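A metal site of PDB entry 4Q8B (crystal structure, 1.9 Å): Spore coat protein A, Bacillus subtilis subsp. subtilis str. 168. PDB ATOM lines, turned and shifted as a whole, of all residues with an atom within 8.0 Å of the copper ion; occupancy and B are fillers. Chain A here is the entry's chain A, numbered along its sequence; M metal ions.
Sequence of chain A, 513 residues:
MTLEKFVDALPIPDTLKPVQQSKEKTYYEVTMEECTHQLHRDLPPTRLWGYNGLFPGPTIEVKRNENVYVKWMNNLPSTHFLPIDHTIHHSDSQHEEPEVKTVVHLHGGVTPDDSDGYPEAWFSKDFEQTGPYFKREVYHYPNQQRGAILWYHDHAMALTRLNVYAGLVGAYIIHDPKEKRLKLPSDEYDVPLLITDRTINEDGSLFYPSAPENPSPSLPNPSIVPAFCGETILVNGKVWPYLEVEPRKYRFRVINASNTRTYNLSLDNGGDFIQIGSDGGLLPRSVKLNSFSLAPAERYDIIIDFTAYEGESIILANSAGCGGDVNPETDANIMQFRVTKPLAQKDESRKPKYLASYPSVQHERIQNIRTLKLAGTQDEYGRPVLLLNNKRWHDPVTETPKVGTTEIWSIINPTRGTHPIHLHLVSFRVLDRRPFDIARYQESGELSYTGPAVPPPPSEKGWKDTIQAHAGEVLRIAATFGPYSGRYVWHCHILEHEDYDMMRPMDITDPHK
A ring nitrogen (ND1) of His 419 lies close to the side-chain sulfur of Met 502, at 3.8 Å.
A ring nitrogen (NE2) of His 419 lies within hydrogen-bond range of the side-chain hydroxyl (OG1) of Thr 415 (2.9 Å).
The backbone carbonyl oxygen (O) of His 419 lies within hydrogen-bond range of the backbone NH (N) of Ala 469.
N of Met 502 sits at hydrogen-bond distance from O of His 497 (2.8 Å).
NE2 of His 497 sits at hydrogen-bond distance from O of Pro 226 (3.0 Å).
The backbone carbonyl oxygen (O) of Met 502 sits at hydrogen-bond distance from the backbone NH (N) of Cys 492.
The side-chain sulfur of Cys 492 sits close to the backbone NH of Ile 494, at 3.4 Å.
The backbone NH of Met 502 lies within hydrogen-bond range of the backbone carbonyl oxygen of Leu 386 (3.1 Å).
Merely in contact with the copper ion: Met 502 and Ile 494.
Five residues have an atom within 4 Å of the copper ion: His 419, Cys 492, Ile 494, His 497 and Met 502.
The copper ion is bound by a ring nitrogen (ND1) of His 419, a ring nitrogen (ND1) of His 497 and the side-chain sulfur (SG) of Cys 492.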
ATOM      1  N   PRO A 226      23.471  -6.680   6.903  1.00  0.00           N
ATOM      2  CA  PRO A 226      22.624  -7.391   7.840  1.00  0.00           C
ATOM      3  C   PRO A 226      23.337  -8.149   8.936  1.00  0.00           C
ATOM      4  O   PRO A 226      22.697  -8.559   9.890  1.00  0.00           O
ATOM      5  CB  PRO A 226      21.860  -8.378   6.971  1.00  0.00           C
ATOM      6  CG  PRO A 226      22.484  -8.374   5.640  1.00  0.00           C
ATOM      7  CD  PRO A 226      23.311  -7.154   5.506  1.00  0.00           C
ATOM      8  N   LEU A 374       9.071 -11.080  16.360  1.00  0.00           N
ATOM      9  CA  LEU A 374      10.259 -10.625  15.619  1.00  0.00           C
ATOM     10  C   LEU A 374       9.901 -10.629  14.131  1.00  0.00           C
ATOM     11  O   LEU A 374       9.645 -11.675  13.528  1.00  0.00           O
ATOM     12  CB  LEU A 374      11.461 -11.481  15.945  1.00  0.00           C
ATOM     13  CG  LEU A 374      11.685 -11.714  17.458  1.00  0.00           C
ATOM     14  CD1 LEU A 374      13.009 -12.423  17.625  1.00  0.00           C
ATOM     15  CD2 LEU A 374      11.643 -10.430  18.297  1.00  0.00           C
ATOM     16  N   LEU A 386      14.985  -5.203  10.144  1.00  0.00           N
ATOM     17  CA  LEU A 386      14.509  -6.037  11.227  1.00  0.00           C
ATOM     18  C   LEU A 386      13.733  -5.235  12.254  1.00  0.00           C
ATOM     19  O   LEU A 386      14.176  -4.166  12.671  1.00  0.00           O
ATOM     20  CB  LEU A 386      15.692  -6.802  11.850  1.00  0.00           C
ATOM     21  CG  LEU A 386      16.019  -8.071  11.043  1.00  0.00           C
ATOM     22  CD1 LEU A 386      17.303  -8.731  11.473  1.00  0.00           C
ATOM     23  CD2 LEU A 386      14.876  -9.093  11.132  1.00  0.00           C
ATOM     24  N   LEU A 387      12.588  -5.752  12.683  1.00  0.00           N
ATOM     25  CA  LEU A 387      11.707  -4.995  13.588  1.00  0.00           C
ATOM     26  C   LEU A 387      11.221  -5.801  14.787  1.00  0.00           C
ATOM     27  O   LEU A 387      11.103  -7.045  14.710  1.00  0.00           O
ATOM     28  CB  LEU A 387      10.495  -4.523  12.838  1.00  0.00           C
ATOM     29  CG  LEU A 387      10.739  -3.762  11.546  1.00  0.00           C
ATOM     30  CD1 LEU A 387       9.412  -3.477  10.884  1.00  0.00           C
ATOM     31  CD2 LEU A 387      11.467  -2.496  11.857  1.00  0.00           C
ATOM     32  N   LEU A 388      10.959  -5.102  15.884  1.00  0.00           N
ATOM     33  CA  LEU A 388      10.327  -5.677  17.076  1.00  0.00           C
ATOM     34  C   LEU A 388       8.817  -5.336  17.045  1.00  0.00           C
ATOM     35  O   LEU A 388       8.406  -4.180  17.066  1.00  0.00           O
ATOM     36  CB  LEU A 388      10.928  -5.146  18.352  1.00  0.00           C
ATOM     37  CG  LEU A 388      12.427  -5.364  18.527  1.00  0.00           C
ATOM     38  CD1 LEU A 388      12.870  -4.557  19.721  1.00  0.00           C
ATOM     39  CD2 LEU A 388      12.733  -6.876  18.708  1.00  0.00           C
ATOM     40  N   ASN A 413       9.579 -15.955  17.302  1.00  0.00           N
ATOM     41  CA  ASN A 413      10.552 -15.751  16.232  1.00  0.00           C
ATOM     42  C   ASN A 413      10.261 -16.615  14.982  1.00  0.00           C
ATOM     43  O   ASN A 413      10.692 -17.764  14.930  1.00  0.00           O
ATOM     44  CB  ASN A 413      11.961 -16.017  16.731  1.00  0.00           C
ATOM     45  CG  ASN A 413      13.024 -15.772  15.679  1.00  0.00           C
ATOM     46  OD1 ASN A 413      12.764 -15.325  14.586  1.00  0.00           O
ATOM     47  ND2 ASN A 413      14.250 -16.100  16.023  1.00  0.00           N
ATOM     48  N   THR A 415      11.601 -15.819  12.011  1.00  0.00           N
ATOM     49  CA  THR A 415      12.665 -15.497  11.064  1.00  0.00           C
ATOM     50  C   THR A 415      13.527 -16.753  10.932  1.00  0.00           C
ATOM     51  O   THR A 415      13.294 -17.765  11.625  1.00  0.00           O
ATOM     52  CB  THR A 415      13.518 -14.288  11.524  1.00  0.00           C
ATOM     53  OG1 THR A 415      14.379 -14.694  12.598  1.00  0.00           O
ATOM     54  CG2 THR A 415      12.636 -13.145  11.982  1.00  0.00           C
ATOM     55  N   GLY A 417      16.771 -16.914  11.628  1.00  0.00           N
ATOM     56  CA  GLY A 417      17.942 -16.902  12.535  1.00  0.00           C
ATOM     57  C   GLY A 417      17.601 -16.660  13.996  1.00  0.00           C
ATOM     58  O   GLY A 417      16.479 -16.341  14.366  1.00  0.00           O
ATOM     59  N   THR A 418      18.616 -16.849  14.834  1.00  0.00           N
ATOM     60  CA  THR A 418      18.538 -16.558  16.233  1.00  0.00           C
ATOM     61  C   THR A 418      18.784 -15.060  16.466  1.00  0.00           C
ATOM     62  O   THR A 418      19.671 -14.462  15.828  1.00  0.00           O
ATOM     63  CB  THR A 418      19.559 -17.389  16.992  1.00  0.00           C
ATOM     64  OG1 THR A 418      19.188 -18.764  16.874  1.00  0.00           O
ATOM     65  CG2 THR A 418      19.587 -17.003  18.492  1.00  0.00           C
ATOM     66  N   HIS A 419      18.001 -14.492  17.373  1.00  0.00           N
ATOM     67  CA  HIS A 419      18.216 -13.119  17.851  1.00  0.00           C
ATOM     68  C   HIS A 419      18.440 -13.104  19.376  1.00  0.00           C
ATOM     69  O   HIS A 419      17.575 -13.567  20.126  1.00  0.00           O
ATOM     70  CB  HIS A 419      17.032 -12.232  17.498  1.00  0.00           C
ATOM     71  CG  HIS A 419      16.700 -12.261  16.050  1.00  0.00           C
ATOM     72  ND1 HIS A 419      17.298 -11.423  15.142  1.00  0.00           N
ATOM     73  CD2 HIS A 419      15.838 -13.037  15.348  1.00  0.00           C
ATOM     74  CE1 HIS A 419      16.842 -11.706  13.921  1.00  0.00           C
ATOM     75  NE2 HIS A 419      15.955 -12.682  14.031  1.00  0.00           N
ATOM     76  N   PRO A 420      19.586 -12.549  19.836  1.00  0.00           N
ATOM     77  CA  PRO A 420      19.835 -12.317  21.227  1.00  0.00           C
ATOM     78  C   PRO A 420      19.150 -11.054  21.715  1.00  0.00           C
ATOM     79  O   PRO A 420      19.637  -9.923  21.500  1.00  0.00           O
ATOM     80  CB  PRO A 420      21.368 -12.222  21.318  1.00  0.00           C
ATOM     81  CG  PRO A 420      21.775 -11.676  19.980  1.00  0.00           C
ATOM     82  CD  PRO A 420      20.708 -12.084  19.004  1.00  0.00           C
ATOM     83  N   ILE A 421      18.021 -11.242  22.364  1.00  0.00           N
ATOM     84  CA  ILE A 421      17.195 -10.162  22.853  1.00  0.00           C
ATOM     85  C   ILE A 421      17.657  -9.701  24.248  1.00  0.00           C
ATOM     86  O   ILE A 421      17.873 -10.496  25.175  1.00  0.00           O
ATOM     87  CB  ILE A 421      15.719 -10.586  22.858  1.00  0.00           C
ATOM     88  CG1 ILE A 421      15.291 -11.112  21.493  1.00  0.00           C
ATOM     89  CG2 ILE A 421      14.839  -9.444  23.420  1.00  0.00           C
ATOM     90  CD1 ILE A 421      15.444 -10.142  20.317  1.00  0.00           C
ATOM     91  N   ALA A 469      16.701 -16.138  21.270  1.00  0.00           N
ATOM     92  CA  ALA A 469      15.372 -16.469  20.749  1.00  0.00           C
ATOM     93  C   ALA A 469      15.609 -17.169  19.433  1.00  0.00           C
ATOM     94  O   ALA A 469      15.907 -16.536  18.394  1.00  0.00           O
ATOM     95  CB  ALA A 469      14.556 -15.221  20.557  1.00  0.00           C
ATOM     96  N   HIS A 491      16.024  -4.509  22.746  1.00  0.00           N
ATOM     97  CA  HIS A 491      16.491  -4.681  21.403  1.00  0.00           C
ATOM     98  C   HIS A 491      17.219  -6.023  21.218  1.00  0.00           C
ATOM     99  O   HIS A 491      17.593  -6.698  22.203  1.00  0.00           O
ATOM    100  CB  HIS A 491      17.465  -3.553  20.984  1.00  0.00           C
ATOM    101  CG  HIS A 491      18.627  -3.366  21.909  1.00  0.00           C
ATOM    102  ND1 HIS A 491      19.865  -3.949  21.696  1.00  0.00           N
ATOM    103  CD2 HIS A 491      18.752  -2.641  23.044  1.00  0.00           C
ATOM    104  CE1 HIS A 491      20.689  -3.602  22.665  1.00  0.00           C
ATOM    105  NE2 HIS A 491      20.045  -2.811  23.489  1.00  0.00           N
ATOM    106  N   CYS A 492      17.357  -6.400  19.959  1.00  0.00           N
ATOM    107  CA  CYS A 492      18.290  -7.440  19.573  1.00  0.00           C
ATOM    108  C   CYS A 492      19.702  -6.892  19.707  1.00  0.00           C
ATOM    109  O   CYS A 492      19.952  -5.742  19.343  1.00  0.00           O
ATOM    110  CB  CYS A 492      18.087  -7.828  18.121  1.00  0.00           C
ATOM    111  SG  CYS A 492      19.239  -9.115  17.546  1.00  0.00           S
ATOM    112  N   HIS A 493      20.611  -7.736  20.222  1.00  0.00           N
ATOM    113  CA  HIS A 493      22.008  -7.318  20.449  1.00  0.00           C
ATOM    114  C   HIS A 493      22.982  -7.740  19.367  1.00  0.00           C
ATOM    115  O   HIS A 493      24.191  -7.541  19.538  1.00  0.00           O
ATOM    116  CB  HIS A 493      22.499  -7.744  21.816  1.00  0.00           C
ATOM    117  CG  HIS A 493      23.432  -6.768  22.454  1.00  0.00           C
ATOM    118  ND1 HIS A 493      24.677  -6.505  21.931  1.00  0.00           N
ATOM    119  CD2 HIS A 493      23.313  -5.989  23.544  1.00  0.00           C
ATOM    120  CE1 HIS A 493      25.285  -5.608  22.673  1.00  0.00           C
ATOM    121  NE2 HIS A 493      24.491  -5.294  23.673  1.00  0.00           N
ATOM    122  N   ILE A 494      22.473  -8.251  18.228  1.00  0.00           N
ATOM    123  CA  ILE A 494      23.256  -8.242  16.992  1.00  0.00           C
ATOM    124  C   ILE A 494      23.255  -6.792  16.512  1.00  0.00           C
ATOM    125  O   ILE A 494      22.166  -6.217  16.203  1.00  0.00           O
ATOM    126  CB  ILE A 494      22.675  -9.193  15.935  1.00  0.00           C
ATOM    127  CG1 ILE A 494      22.860 -10.684  16.338  1.00  0.00           C
ATOM    128  CG2 ILE A 494      23.287  -8.951  14.596  1.00  0.00           C
ATOM    129  CD1 ILE A 494      21.983 -11.651  15.537  1.00  0.00           C
ATOM    130  N   LEU A 495      24.424  -6.156  16.500  1.00  0.00           N
ATOM    131  CA  LEU A 495      24.411  -4.705  16.380  1.00  0.00           C
ATOM    132  C   LEU A 495      23.943  -4.243  15.027  1.00  0.00           C
ATOM    133  O   LEU A 495      23.335  -3.133  14.886  1.00  0.00           O
ATOM    134  CB  LEU A 495      25.777  -4.094  16.722  1.00  0.00           C
ATOM    135  CG  LEU A 495      26.262  -4.467  18.117  1.00  0.00           C
ATOM    136  CD1 LEU A 495      27.626  -3.815  18.387  1.00  0.00           C
ATOM    137  CD2 LEU A 495      25.305  -4.066  19.185  1.00  0.00           C
ATOM    138  N   GLU A 496      24.220  -5.035  13.995  1.00  0.00           N
ATOM    139  CA  GLU A 496      23.697  -4.775  12.676  1.00  0.00           C
ATOM    140  C   GLU A 496      22.139  -4.807  12.619  1.00  0.00           C
ATOM    141  O   GLU A 496      21.518  -4.099  11.801  1.00  0.00           O
ATOM    142  CB  GLU A 496      24.275  -5.785  11.673  1.00  0.00           C
ATOM    143  CG  GLU A 496      25.730  -5.432  11.280  1.00  0.00           C
ATOM    144  CD  GLU A 496      26.764  -5.698  12.377  1.00  0.00           C
ATOM    145  OE1 GLU A 496      26.520  -6.527  13.282  1.00  0.00           O
ATOM    146  OE2 GLU A 496      27.850  -5.047  12.312  1.00  0.00           O
ATOM    147  N   HIS A 497      21.518  -5.549  13.512  1.00  0.00           N
ATOM    148  CA  HIS A 497      20.040  -5.569  13.583  1.00  0.00           C
ATOM    149  C   HIS A 497      19.507  -4.411  14.430  1.00  0.00           C
ATOM    150  O   HIS A 497      18.570  -3.665  14.030  1.00  0.00           O
ATOM    151  CB  HIS A 497      19.587  -6.888  14.198  1.00  0.00           C
ATOM    152  CG  HIS A 497      19.929  -8.083  13.354  1.00  0.00           C
ATOM    153  ND1 HIS A 497      19.573  -9.368  13.700  1.00  0.00           N
ATOM    154  CD2 HIS A 497      20.599  -8.190  12.178  1.00  0.00           C
ATOM    155  CE1 HIS A 497      19.981 -10.217  12.787  1.00  0.00           C
ATOM    156  NE2 HIS A 497      20.614  -9.523  11.845  1.00  0.00           N
ATOM    157  N   GLU A 498      20.119  -4.251  15.602  1.00  0.00           N
ATOM    158  CA  GLU A 498      19.872  -3.121  16.501  1.00  0.00           C
ATOM    159  C   GLU A 498      19.795  -1.795  15.745  1.00  0.00           C
ATOM    160  O   GLU A 498      18.861  -1.020  15.979  1.00  0.00           O
ATOM    161  CB  GLU A 498      20.970  -3.055  17.563  1.00  0.00           C
ATOM    162  CG  GLU A 498      20.716  -2.016  18.650  1.00  0.00           C
ATOM    163  CD  GLU A 498      21.804  -2.001  19.714  1.00  0.00           C
ATOM    164  OE1 GLU A 498      22.412  -3.068  20.008  1.00  0.00           O
ATOM    165  OE2 GLU A 498      22.014  -0.898  20.277  1.00  0.00           O
ATOM    166  N   MET A 502      15.977  -2.918  14.931  1.00  0.00           N
ATOM    167  CA  MET A 502      15.433  -3.869  15.892  1.00  0.00           C
ATOM    168  C   MET A 502      15.655  -3.417  17.319  1.00  0.00           C
ATOM    169  O   MET A 502      16.279  -4.150  18.133  1.00  0.00           O
ATOM    170  CB  MET A 502      16.100  -5.211  15.629  1.00  0.00           C
ATOM    171  CG  MET A 502      15.284  -6.412  16.038  1.00  0.00           C
ATOM    172  SD  MET A 502      15.876  -7.959  15.375  1.00  0.00           S
ATOM    173  CE  MET A 502      14.587  -8.961  16.055  1.00  0.00           C
HETATM  174 CU    CU M   1      18.650  -9.846  15.545  1.00  0.00          CU
